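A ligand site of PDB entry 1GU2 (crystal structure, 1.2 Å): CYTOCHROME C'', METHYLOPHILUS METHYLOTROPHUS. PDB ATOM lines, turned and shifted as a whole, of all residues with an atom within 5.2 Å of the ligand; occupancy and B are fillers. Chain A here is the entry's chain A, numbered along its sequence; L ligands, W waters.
Water W5 bridges an oxygen (O1) of the ligand (2.5 Å) and the side-chain carboxylate of Asp 84 (2.5 Å). Water W7 lies within hydrogen-bond range of O2 of the ligand, OD1 of Asp 84 and N of Phe 82. Water W6 bridges O3 of the ligand (2.7 Å) and NH2 of Arg 81 (3.4 Å).
Merely in contact with the ligand: Pro 71 (3.4 Å), Glu 91 (3.5 Å), Asn 63 (3.5 Å), Leu 73 (3.6 Å), Ala 48 (3.6 Å), Phe 34 (3.7 Å), Ile 99 (3.7 Å), Ile 70 (3.7 Å), Val 88 (3.7 Å), Phe 112 (3.9 Å) and Leu 100 (3.9 Å). Hydrophobic or aromatic side chains within 4 Å of the ligand: Phe 34, His 53, Ile 70, Pro 71, Leu 73, Val 88, His 95, Ile 99, Leu 100 and Phe 112. 16 residues have an atom within 4 Å of the ligand: Phe 34, Ala 48, Cys 49, Cys 52, His 53, Asn 63, Ile 70, Pro 71, Leu 73, Arg 81, Val 88, Glu 91, His 95, Ile 99, Leu 100 and Phe 112.
The side-chain amide nitrogen of Asn 63 sits close to the backbone NH of Val 65 (3.2 Å). NH1 of Arg 81 lies within hydrogen-bond range of O of Pro 71. SG of Cys 52 is in hydrogen-bond range of N of Ile 64 (3.5 Å). The backbone NH (N) of Cys 49 lies close to the backbone carbonyl oxygen (O) of Phe 35. N of Ala 48 is in hydrogen-bond range of OG of Ser 51 (2.9 Å).
The guanidinium group (NH2) of Arg 81 lies within salt-bridge range of an oxygen (O4) of the ligand (2.9 Å). C25 of the ligand is bonded to SG of Cys 52 (1.9 Å). A carbon (C18) of the ligand is bonded to the side-chain sulfur (SG) of Cys 49 (1.8 Å). NE2 of His 95 is bound to FE1 of the ligand (2.0 Å). FE1 of the ligand is bound by NE2 of His 53, at 2.0 Å.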
ATOM      1  N   PHE A  34      -1.316  27.528   7.385  1.00  0.00           N
ATOM      2  CA  PHE A  34      -1.521  26.091   7.251  1.00  0.00           C
ATOM      3  C   PHE A  34      -2.957  25.736   7.609  1.00  0.00           C
ATOM      4  O   PHE A  34      -3.623  24.954   6.937  1.00  0.00           O
ATOM      5  CB  PHE A  34      -0.520  25.391   8.153  1.00  0.00           C
ATOM      6  CG  PHE A  34      -0.760  23.917   8.400  1.00  0.00           C
ATOM      7  CD1 PHE A  34      -1.436  23.516   9.561  1.00  0.00           C
ATOM      8  CD2 PHE A  34      -0.317  22.969   7.497  1.00  0.00           C
ATOM      9  CE1 PHE A  34      -1.618  22.187   9.852  1.00  0.00           C
ATOM     10  CE2 PHE A  34      -0.495  21.618   7.790  1.00  0.00           C
ATOM     11  CZ  PHE A  34      -1.172  21.275   8.939  1.00  0.00           C
ATOM     12  N   PHE A  35      -3.505  26.313   8.670  1.00  0.00           N
ATOM     13  CA  PHE A  35      -4.863  26.014   9.167  1.00  0.00           C
ATOM     14  C   PHE A  35      -5.946  26.440   8.193  1.00  0.00           C
ATOM     15  O   PHE A  35      -6.972  25.756   8.103  1.00  0.00           O
ATOM     16  CB  PHE A  35      -5.024  26.695  10.534  1.00  0.00           C
ATOM     17  CG  PHE A  35      -6.326  26.458  11.237  1.00  0.00           C
ATOM     18  CD1 PHE A  35      -6.687  25.199  11.731  1.00  0.00           C
ATOM     19  CD2 PHE A  35      -7.224  27.507  11.428  1.00  0.00           C
ATOM     20  CE1 PHE A  35      -7.911  24.991  12.360  1.00  0.00           C
ATOM     21  CE2 PHE A  35      -8.445  27.323  12.077  1.00  0.00           C
ATOM     22  CZ  PHE A  35      -8.783  26.056  12.537  1.00  0.00           C
ATOM     23  N   PHE A  39      -6.550  23.126   0.354  1.00  0.00           N
ATOM     24  CA  PHE A  39      -5.849  22.053  -0.350  1.00  0.00           C
ATOM     25  C   PHE A  39      -6.838  21.322  -1.225  1.00  0.00           C
ATOM     26  O   PHE A  39      -8.057  21.460  -1.121  1.00  0.00           O
ATOM     27  CB  PHE A  39      -5.162  21.124   0.668  1.00  0.00           C
ATOM     28  CG  PHE A  39      -6.055  20.578   1.751  1.00  0.00           C
ATOM     29  CD1 PHE A  39      -6.940  19.532   1.521  1.00  0.00           C
ATOM     30  CD2 PHE A  39      -5.976  21.090   3.037  1.00  0.00           C
ATOM     31  CE1 PHE A  39      -7.722  18.994   2.557  1.00  0.00           C
ATOM     32  CE2 PHE A  39      -6.752  20.604   4.079  1.00  0.00           C
ATOM     33  CZ  PHE A  39      -7.638  19.548   3.845  1.00  0.00           C
ATOM     34  N   ALA A  48     -10.040  22.820   3.812  1.00  0.00           N
ATOM     35  CA  ALA A  48      -9.008  23.351   4.710  1.00  0.00           C
ATOM     36  C   ALA A  48      -9.276  22.801   6.108  1.00  0.00           C
ATOM     37  O   ALA A  48     -10.385  22.359   6.396  1.00  0.00           O
ATOM     38  CB  ALA A  48      -9.042  24.879   4.793  1.00  0.00           C
ATOM     39  N   CYS A  49      -8.296  22.868   6.987  1.00  0.00           N
ATOM     40  CA  CYS A  49      -8.588  22.539   8.397  1.00  0.00           C
ATOM     41  C   CYS A  49      -9.801  23.366   8.911  1.00  0.00           C
ATOM     42  O   CYS A  49     -10.645  22.844   9.648  1.00  0.00           O
ATOM     43  CB  CYS A  49      -7.395  22.813   9.299  1.00  0.00           C
ATOM     44  SG  CYS A  49      -5.802  22.180   8.733  1.00  0.00           S
ATOM     45  N   SER A  51     -12.351  24.207   7.355  1.00  0.00           N
ATOM     46  CA  SER A  51     -13.634  23.745   6.865  1.00  0.00           C
ATOM     47  C   SER A  51     -14.456  23.107   7.967  1.00  0.00           C
ATOM     48  O   SER A  51     -15.660  23.273   7.997  1.00  0.00           O
ATOM     49  CB  SER A  51     -13.477  22.721   5.754  1.00  0.00           C
ATOM     50  OG  SER A  51     -12.824  23.275   4.614  1.00  0.00           O
ATOM     51  N   CYS A  52     -13.770  22.357   8.850  1.00  0.00           N
ATOM     52  CA  CYS A  52     -14.425  21.702   9.976  1.00  0.00           C
ATOM     53  C   CYS A  52     -14.219  22.460  11.264  1.00  0.00           C
ATOM     54  O   CYS A  52     -15.095  22.489  12.127  1.00  0.00           O
ATOM     55  CB  CYS A  52     -13.900  20.265  10.122  1.00  0.00           C
ATOM     56  SG  CYS A  52     -14.374  19.259   8.715  1.00  0.00           S
ATOM     57  N   HIS A  53     -13.057  23.084  11.463  1.00  0.00           N
ATOM     58  CA  HIS A  53     -12.736  23.681  12.785  1.00  0.00           C
ATOM     59  C   HIS A  53     -13.078  25.144  12.831  1.00  0.00           C
ATOM     60  O   HIS A  53     -12.874  25.795  13.865  1.00  0.00           O
ATOM     61  CB  HIS A  53     -11.238  23.425  13.089  1.00  0.00           C
ATOM     62  CG  HIS A  53     -10.954  21.971  13.303  1.00  0.00           C
ATOM     63  ND1 HIS A  53     -11.424  21.268  14.391  1.00  0.00           N
ATOM     64  CD2 HIS A  53     -10.233  21.067  12.632  1.00  0.00           C
ATOM     65  CE1 HIS A  53     -10.988  19.997  14.349  1.00  0.00           C
ATOM     66  NE2 HIS A  53     -10.265  19.841  13.280  1.00  0.00           N
ATOM     67  N   ASN A  63     -18.150  18.936  11.786  1.00  0.00           N
ATOM     68  CA  ASN A  63     -17.608  18.000  10.796  1.00  0.00           C
ATOM     69  C   ASN A  63     -18.443  18.100   9.534  1.00  0.00           C
ATOM     70  O   ASN A  63     -19.635  17.801   9.578  1.00  0.00           O
ATOM     71  CB  ASN A  63     -17.655  16.634  11.475  1.00  0.00           C
ATOM     72  CG  ASN A  63     -16.960  15.474  10.888  1.00  0.00           C
ATOM     73  OD1 ASN A  63     -16.454  14.469  11.391  1.00  0.00           O
ATOM     74  ND2 ASN A  63     -16.868  15.597   9.596  1.00  0.00           N
ATOM     75  N   ILE A  64     -17.788  18.424   8.408  1.00  0.00           N
ATOM     76  CA  ILE A  64     -18.564  18.603   7.166  1.00  0.00           C
ATOM     77  C   ILE A  64     -19.063  17.309   6.583  1.00  0.00           C
ATOM     78  O   ILE A  64     -20.003  17.296   5.788  1.00  0.00           O
ATOM     79  CB  ILE A  64     -17.718  19.330   6.110  1.00  0.00           C
ATOM     80  CG1 ILE A  64     -16.475  18.585   5.661  1.00  0.00           C
ATOM     81  CG2 ILE A  64     -17.420  20.704   6.727  1.00  0.00           C
ATOM     82  CD1 ILE A  64     -15.678  19.191   4.499  1.00  0.00           C
ATOM     83  N   VAL A  65     -18.492  16.182   6.872  1.00  0.00           N
ATOM     84  CA  VAL A  65     -18.937  14.829   6.506  1.00  0.00           C
ATOM     85  C   VAL A  65     -20.136  14.381   7.319  1.00  0.00           C
ATOM     86  O   VAL A  65     -21.074  13.895   6.675  1.00  0.00           O
ATOM     87  CB  VAL A  65     -17.797  13.822   6.638  1.00  0.00           C
ATOM     88  CG1 VAL A  65     -18.229  12.422   6.227  1.00  0.00           C
ATOM     89  CG2 VAL A  65     -16.617  14.290   5.772  1.00  0.00           C
ATOM     90  N   ILE A  70     -17.771  19.736  16.895  1.00  0.00           N
ATOM     91  CA  ILE A  70     -16.416  19.438  17.336  1.00  0.00           C
ATOM     92  C   ILE A  70     -15.969  20.420  18.407  1.00  0.00           C
ATOM     93  O   ILE A  70     -15.984  21.610  18.168  1.00  0.00           O
ATOM     94  CB  ILE A  70     -15.432  19.482  16.170  1.00  0.00           C
ATOM     95  CG1 ILE A  70     -15.858  18.650  14.956  1.00  0.00           C
ATOM     96  CG2 ILE A  70     -14.084  19.000  16.646  1.00  0.00           C
ATOM     97  CD1 ILE A  70     -15.058  18.983  13.726  1.00  0.00           C
ATOM     98  N   PRO A  71     -15.585  19.986  19.605  1.00  0.00           N
ATOM     99  CA  PRO A  71     -15.119  20.964  20.600  1.00  0.00           C
ATOM    100  C   PRO A  71     -13.956  21.798  20.067  1.00  0.00           C
ATOM    101  O   PRO A  71     -13.177  21.384  19.175  1.00  0.00           O
ATOM    102  CB  PRO A  71     -14.688  20.047  21.748  1.00  0.00           C
ATOM    103  CG  PRO A  71     -15.604  18.851  21.631  1.00  0.00           C
ATOM    104  CD  PRO A  71     -15.644  18.621  20.109  1.00  0.00           C
ATOM    105  N   LEU A  73     -10.343  23.551  19.418  1.00  0.00           N
ATOM    106  CA  LEU A  73      -8.956  23.096  19.452  1.00  0.00           C
ATOM    107  C   LEU A  73      -8.023  23.891  20.381  1.00  0.00           C
ATOM    108  O   LEU A  73      -7.047  23.340  20.886  1.00  0.00           O
ATOM    109  CB  LEU A  73      -8.370  23.127  18.051  1.00  0.00           C
ATOM    110  CG  LEU A  73      -9.065  22.222  16.996  1.00  0.00           C
ATOM    111  CD1 LEU A  73      -8.276  22.238  15.698  1.00  0.00           C
ATOM    112  CD2 LEU A  73      -9.253  20.799  17.536  1.00  0.00           C
ATOM    113  N   ARG A  81      -7.895  19.708  25.610  1.00  0.00           N
ATOM    114  CA  ARG A  81      -6.968  19.489  24.490  1.00  0.00           C
ATOM    115  C   ARG A  81      -5.536  19.358  24.943  1.00  0.00           C
ATOM    116  O   ARG A  81      -5.023  20.255  25.644  1.00  0.00           O
ATOM    117  CB  ARG A  81      -7.107  20.614  23.450  1.00  0.00           C
ATOM    118  CG  ARG A  81      -8.469  20.716  22.736  1.00  0.00           C
ATOM    119  CD  ARG A  81      -8.775  19.441  21.968  1.00  0.00           C
ATOM    120  NE  ARG A  81      -9.988  19.613  21.182  1.00  0.00           N
ATOM    121  CZ  ARG A  81     -10.595  18.605  20.575  1.00  0.00           C
ATOM    122  NH1 ARG A  81     -11.680  18.868  19.867  1.00  0.00           N
ATOM    123  NH2 ARG A  81     -10.135  17.370  20.695  1.00  0.00           N
ATOM    124  N   PHE A  82      -4.886  18.265  24.576  1.00  0.00           N
ATOM    125  CA  PHE A  82      -3.505  17.914  24.875  1.00  0.00           C
ATOM    126  C   PHE A  82      -3.285  17.414  26.299  1.00  0.00           C
ATOM    127  O   PHE A  82      -2.131  17.064  26.646  1.00  0.00           O
ATOM    128  CB  PHE A  82      -2.478  19.000  24.519  1.00  0.00           C
ATOM    129  CG  PHE A  82      -2.583  19.485  23.083  1.00  0.00           C
ATOM    130  CD1 PHE A  82      -3.294  20.642  22.764  1.00  0.00           C
ATOM    131  CD2 PHE A  82      -1.984  18.764  22.062  1.00  0.00           C
ATOM    132  CE1 PHE A  82      -3.418  21.070  21.449  1.00  0.00           C
ATOM    133  CE2 PHE A  82      -2.095  19.181  20.749  1.00  0.00           C
ATOM    134  CZ  PHE A  82      -2.859  20.311  20.417  1.00  0.00           C
ATOM    135  N   ASP A  84      -4.335  14.545  27.476  1.00  0.00           N
ATOM    136  CA  ASP A  84      -4.192  13.116  27.277  1.00  0.00           C
ATOM    137  C   ASP A  84      -2.859  12.881  26.580  1.00  0.00           C
ATOM    138  O   ASP A  84      -2.758  12.390  25.473  1.00  0.00           O
ATOM    139  CB  ASP A  84      -5.321  12.524  26.482  1.00  0.00           C
ATOM    140  CG  ASP A  84      -5.564  13.154  25.138  1.00  0.00           C
ATOM    141  OD1 ASP A  84      -5.226  14.322  24.910  1.00  0.00           O
ATOM    142  OD2 ASP A  84      -6.180  12.462  24.257  1.00  0.00           O
ATOM    143  N   VAL A  88      -2.072  11.844  22.653  1.00  0.00           N
ATOM    144  CA  VAL A  88      -2.425  12.889  21.705  1.00  0.00           C
ATOM    145  C   VAL A  88      -1.451  12.961  20.552  1.00  0.00           C
ATOM    146  O   VAL A  88      -1.800  13.340  19.445  1.00  0.00           O
ATOM    147  CB  VAL A  88      -2.569  14.244  22.417  1.00  0.00           C
ATOM    148  CG1 VAL A  88      -1.191  14.727  22.914  1.00  0.00           C
ATOM    149  CG2 VAL A  88      -3.245  15.262  21.505  1.00  0.00           C
ATOM    150  N   GLU A  91      -2.603  10.377  18.206  1.00  0.00           N
ATOM    151  CA  GLU A  91      -3.903  10.775  17.613  1.00  0.00           C
ATOM    152  C   GLU A  91      -3.712  11.855  16.563  1.00  0.00           C
ATOM    153  O   GLU A  91      -4.404  11.844  15.546  1.00  0.00           O
ATOM    154  CB  GLU A  91      -4.870  11.229  18.734  1.00  0.00           C
ATOM    155  CG  GLU A  91      -5.208  10.097  19.660  1.00  0.00           C
ATOM    156  CD  GLU A  91      -6.133   9.027  19.121  1.00  0.00           C
ATOM    157  OE1 GLU A  91      -6.834   9.250  18.105  1.00  0.00           O
ATOM    158  OE2 GLU A  91      -6.145   7.935  19.755  1.00  0.00           O
ATOM    159  N   PHE A  92      -2.797  12.801  16.778  1.00  0.00           N
ATOM    160  CA  PHE A  92      -2.572  13.856  15.796  1.00  0.00           C
ATOM    161  C   PHE A  92      -1.941  13.292  14.530  1.00  0.00           C
ATOM    162  O   PHE A  92      -2.331  13.651  13.418  1.00  0.00           O
ATOM    163  CB  PHE A  92      -1.691  14.952  16.406  1.00  0.00           C
ATOM    164  CG  PHE A  92      -1.602  16.286  15.643  1.00  0.00           C
ATOM    165  CD1 PHE A  92      -2.416  16.655  14.631  1.00  0.00           C
ATOM    166  CD2 PHE A  92      -0.669  17.204  16.044  1.00  0.00           C
ATOM    167  CE1 PHE A  92      -2.358  17.887  13.998  1.00  0.00           C
ATOM    168  CE2 PHE A  92      -0.554  18.458  15.468  1.00  0.00           C
ATOM    169  CZ  PHE A  92      -1.399  18.790  14.441  1.00  0.00           C
ATOM    170  N   HIS A  95      -4.756  11.642  12.684  1.00  0.00           N
ATOM    171  CA  HIS A  95      -5.654  12.650  12.073  1.00  0.00           C
ATOM    172  C   HIS A  95      -5.050  13.298  10.850  1.00  0.00           C
ATOM    173  O   HIS A  95      -5.713  13.487   9.841  1.00  0.00           O
ATOM    174  CB  HIS A  95      -5.999  13.700  13.136  1.00  0.00           C
ATOM    175  CG  HIS A  95      -7.102  14.632  12.751  1.00  0.00           C
ATOM    176  ND1 HIS A  95      -8.326  14.192  12.259  1.00  0.00           N
ATOM    177  CD2 HIS A  95      -7.219  15.969  12.827  1.00  0.00           C
ATOM    178  CE1 HIS A  95      -9.121  15.228  12.061  1.00  0.00           C
ATOM    179  NE2 HIS A  95      -8.461  16.345  12.409  1.00  0.00           N
ATOM    180  N   ILE A  99      -6.811  13.220   7.131  1.00  0.00           N
ATOM    181  CA  ILE A  99      -7.208  14.414   6.411  1.00  0.00           C
ATOM    182  C   ILE A  99      -6.347  14.665   5.173  1.00  0.00           C
ATOM    183  O   ILE A  99      -6.869  15.035   4.113  1.00  0.00           O
ATOM    184  CB  ILE A  99      -7.172  15.632   7.378  1.00  0.00           C
ATOM    185  CG1 ILE A  99      -8.110  15.508   8.588  1.00  0.00           C
ATOM    186  CG2 ILE A  99      -7.412  16.926   6.627  1.00  0.00           C
ATOM    187  CD1 ILE A  99      -9.548  15.193   8.242  1.00  0.00           C
ATOM    188  N   LEU A 100      -5.017  14.471   5.336  1.00  0.00           N
ATOM    189  CA  LEU A 100      -4.091  14.873   4.266  1.00  0.00           C
ATOM    190  C   LEU A 100      -3.494  13.716   3.500  1.00  0.00           C
ATOM    191  O   LEU A 100      -2.889  13.947   2.448  1.00  0.00           O
ATOM    192  CB  LEU A 100      -2.993  15.728   4.900  1.00  0.00           C
ATOM    193  CG  LEU A 100      -3.396  17.031   5.572  1.00  0.00           C
ATOM    194  CD1 LEU A 100      -2.201  17.673   6.261  1.00  0.00           C
ATOM    195  CD2 LEU A 100      -4.052  17.986   4.597  1.00  0.00           C
ATOM    196  N   CYS A 104       1.478  15.060   9.334  1.00  0.00           N
ATOM    197  CA  CYS A 104       1.965  16.460   9.206  1.00  0.00           C
ATOM    198  C   CYS A 104       3.435  16.435   9.550  1.00  0.00           C
ATOM    199  O   CYS A 104       3.910  15.556  10.314  1.00  0.00           O
ATOM    200  CB  CYS A 104       1.171  17.337  10.175  1.00  0.00           C
ATOM    201  SG  CYS A 104      -0.647  17.401   9.913  1.00  0.00           S
ATOM    202  N   PHE A 112       1.657  24.953  14.062  1.00  0.00           N
ATOM    203  CA  PHE A 112       0.230  24.907  14.307  1.00  0.00           C
ATOM    204  C   PHE A 112      -0.085  24.972  15.804  1.00  0.00           C
ATOM    205  O   PHE A 112      -0.977  25.702  16.190  1.00  0.00           O
ATOM    206  CB  PHE A 112      -0.364  23.644  13.668  1.00  0.00           C
ATOM    207  CG  PHE A 112      -1.843  23.528  13.984  1.00  0.00           C
ATOM    208  CD1 PHE A 112      -2.309  22.497  14.779  1.00  0.00           C
ATOM    209  CD2 PHE A 112      -2.712  24.468  13.472  1.00  0.00           C
ATOM    210  CE1 PHE A 112      -3.662  22.403  15.070  1.00  0.00           C
ATOM    211  CE2 PHE A 112      -4.047  24.423  13.774  1.00  0.00           C
ATOM    212  CZ  PHE A 112      -4.491  23.382  14.570  1.00  0.00           C
ATOM    213  N   LEU A 116      -2.154  27.736  17.904  1.00  0.00           N
ATOM    214  CA  LEU A 116      -3.248  27.452  18.852  1.00  0.00           C
ATOM    215  C   LEU A 116      -3.042  28.169  20.192  1.00  0.00           C
ATOM    216  O   LEU A 116      -4.074  28.596  20.785  1.00  0.00           O
ATOM    217  CB  LEU A 116      -3.377  25.974  19.115  1.00  0.00           C
ATOM    218  CG  LEU A 116      -3.901  25.072  18.000  1.00  0.00           C
ATOM    219  CD1 LEU A 116      -4.016  23.643  18.501  1.00  0.00           C
ATOM    220  CD2 LEU A 116      -5.236  25.518  17.449  1.00  0.00           C
HETATM  221 FE1  LIG L   1      -9.337  18.108  12.835  1.00  0.00          FE
HETATM  222  C1  LIG L   1      -9.704  16.693  15.938  1.00  0.00           C
HETATM  223  C2  LIG L   1      -6.389  19.498  13.840  1.00  0.00           C
HETATM  224  C3  LIG L   1      -8.742  19.084   9.600  1.00  0.00           C
HETATM  225  C4  LIG L   1     -12.468  16.996  11.964  1.00  0.00           C
HETATM  226  N1  LIG L   1      -8.296  18.160  14.552  1.00  0.00           N
HETATM  227  C5  LIG L   1      -8.590  17.494  15.748  1.00  0.00           C
HETATM  228  C6  LIG L   1      -7.555  17.763  16.716  1.00  0.00           C
HETATM  229  C7  LIG L   1      -6.665  18.584  16.152  1.00  0.00           C
HETATM  230  C8  LIG L   1      -7.093  18.802  14.789  1.00  0.00           C
HETATM  231  C9  LIG L   1      -5.370  19.172  16.763  1.00  0.00           C
HETATM  232  C10 LIG L   1      -7.535  17.193  18.151  1.00  0.00           C
HETATM  233  C11 LIG L   1      -6.736  15.876  18.243  1.00  0.00           C
HETATM  234  C12 LIG L   1      -6.725  15.317  19.618  1.00  0.00           C
HETATM  235  O1  LIG L   1      -6.670  14.080  19.758  1.00  0.00           O
HETATM  236  O2  LIG L   1      -6.778  16.065  20.611  1.00  0.00           O
HETATM  237  N2  LIG L   1      -7.849  19.082  11.912  1.00  0.00           N
HETATM  238  C13 LIG L   1      -6.702  19.557  12.478  1.00  0.00           C
HETATM  239  C14 LIG L   1      -5.838  20.097  11.437  1.00  0.00           C
HETATM  240  C15 LIG L   1      -6.481  19.956  10.253  1.00  0.00           C
HETATM  241  C16 LIG L   1      -7.752  19.336  10.555  1.00  0.00           C
HETATM  242  C17 LIG L   1      -4.435  20.714  11.660  1.00  0.00           C
HETATM  243  C18 LIG L   1      -6.035  20.368   8.830  1.00  0.00           C
HETATM  244  C19 LIG L   1      -4.732  19.681   8.425  1.00  0.00           C
HETATM  245  N3  LIG L   1     -10.393  18.059  11.135  1.00  0.00           N
HETATM  246  C20 LIG L   1      -9.993  18.548   9.903  1.00  0.00           C
HETATM  247  C21 LIG L   1     -11.086  18.462   8.957  1.00  0.00           C
HETATM  248  C22 LIG L   1     -12.148  17.891   9.618  1.00  0.00           C
HETATM  249  C23 LIG L   1     -11.719  17.636  10.968  1.00  0.00           C
HETATM  250  C24 LIG L   1     -10.986  18.982   7.517  1.00  0.00           C
HETATM  251  C25 LIG L   1     -13.579  17.643   9.148  1.00  0.00           C
HETATM  252  C26 LIG L   1     -13.666  16.749   7.914  1.00  0.00           C
HETATM  253  N4  LIG L   1     -10.773  17.069  13.760  1.00  0.00           N
HETATM  254  C27 LIG L   1     -11.997  16.671  13.217  1.00  0.00           C
HETATM  255  C28 LIG L   1     -12.667  15.777  14.125  1.00  0.00           C
HETATM  256  C29 LIG L   1     -11.810  15.547  15.163  1.00  0.00           C
HETATM  257  C30 LIG L   1     -10.688  16.443  15.005  1.00  0.00           C
HETATM  258  C31 LIG L   1     -14.067  15.175  13.917  1.00  0.00           C
HETATM  259  C32 LIG L   1     -11.995  14.468  16.268  1.00  0.00           C
HETATM  260  C33 LIG L   1     -13.046  14.868  17.331  1.00  0.00           C
HETATM  261  C34 LIG L   1     -12.477  15.632  18.502  1.00  0.00           C
HETATM  262  O3  LIG L   1     -13.225  16.367  19.221  1.00  0.00           O
HETATM  263  O4  LIG L   1     -11.253  15.517  18.765  1.00  0.00           O
HETATM  264  O   HOH W   1      -9.434  13.544  18.644  1.00  0.00           O
HETATM  265  O   HOH W   2      -6.357  20.861  19.631  1.00  0.00           O
HETATM  266  O   HOH W   3      -5.342  18.516  20.817  1.00  0.00           O
HETATM  267  O   HOH W   4     -15.644  15.297  19.203  1.00  0.00           O
HETATM  268  O   HOH W   5      -6.112  12.542  21.710  1.00  0.00           O
HETATM  269  O   HOH W   6     -13.115  16.224  21.940  1.00  0.00           O
HETATM  270  O   HOH W   7      -6.392  16.164  23.265  1.00  0.00           O
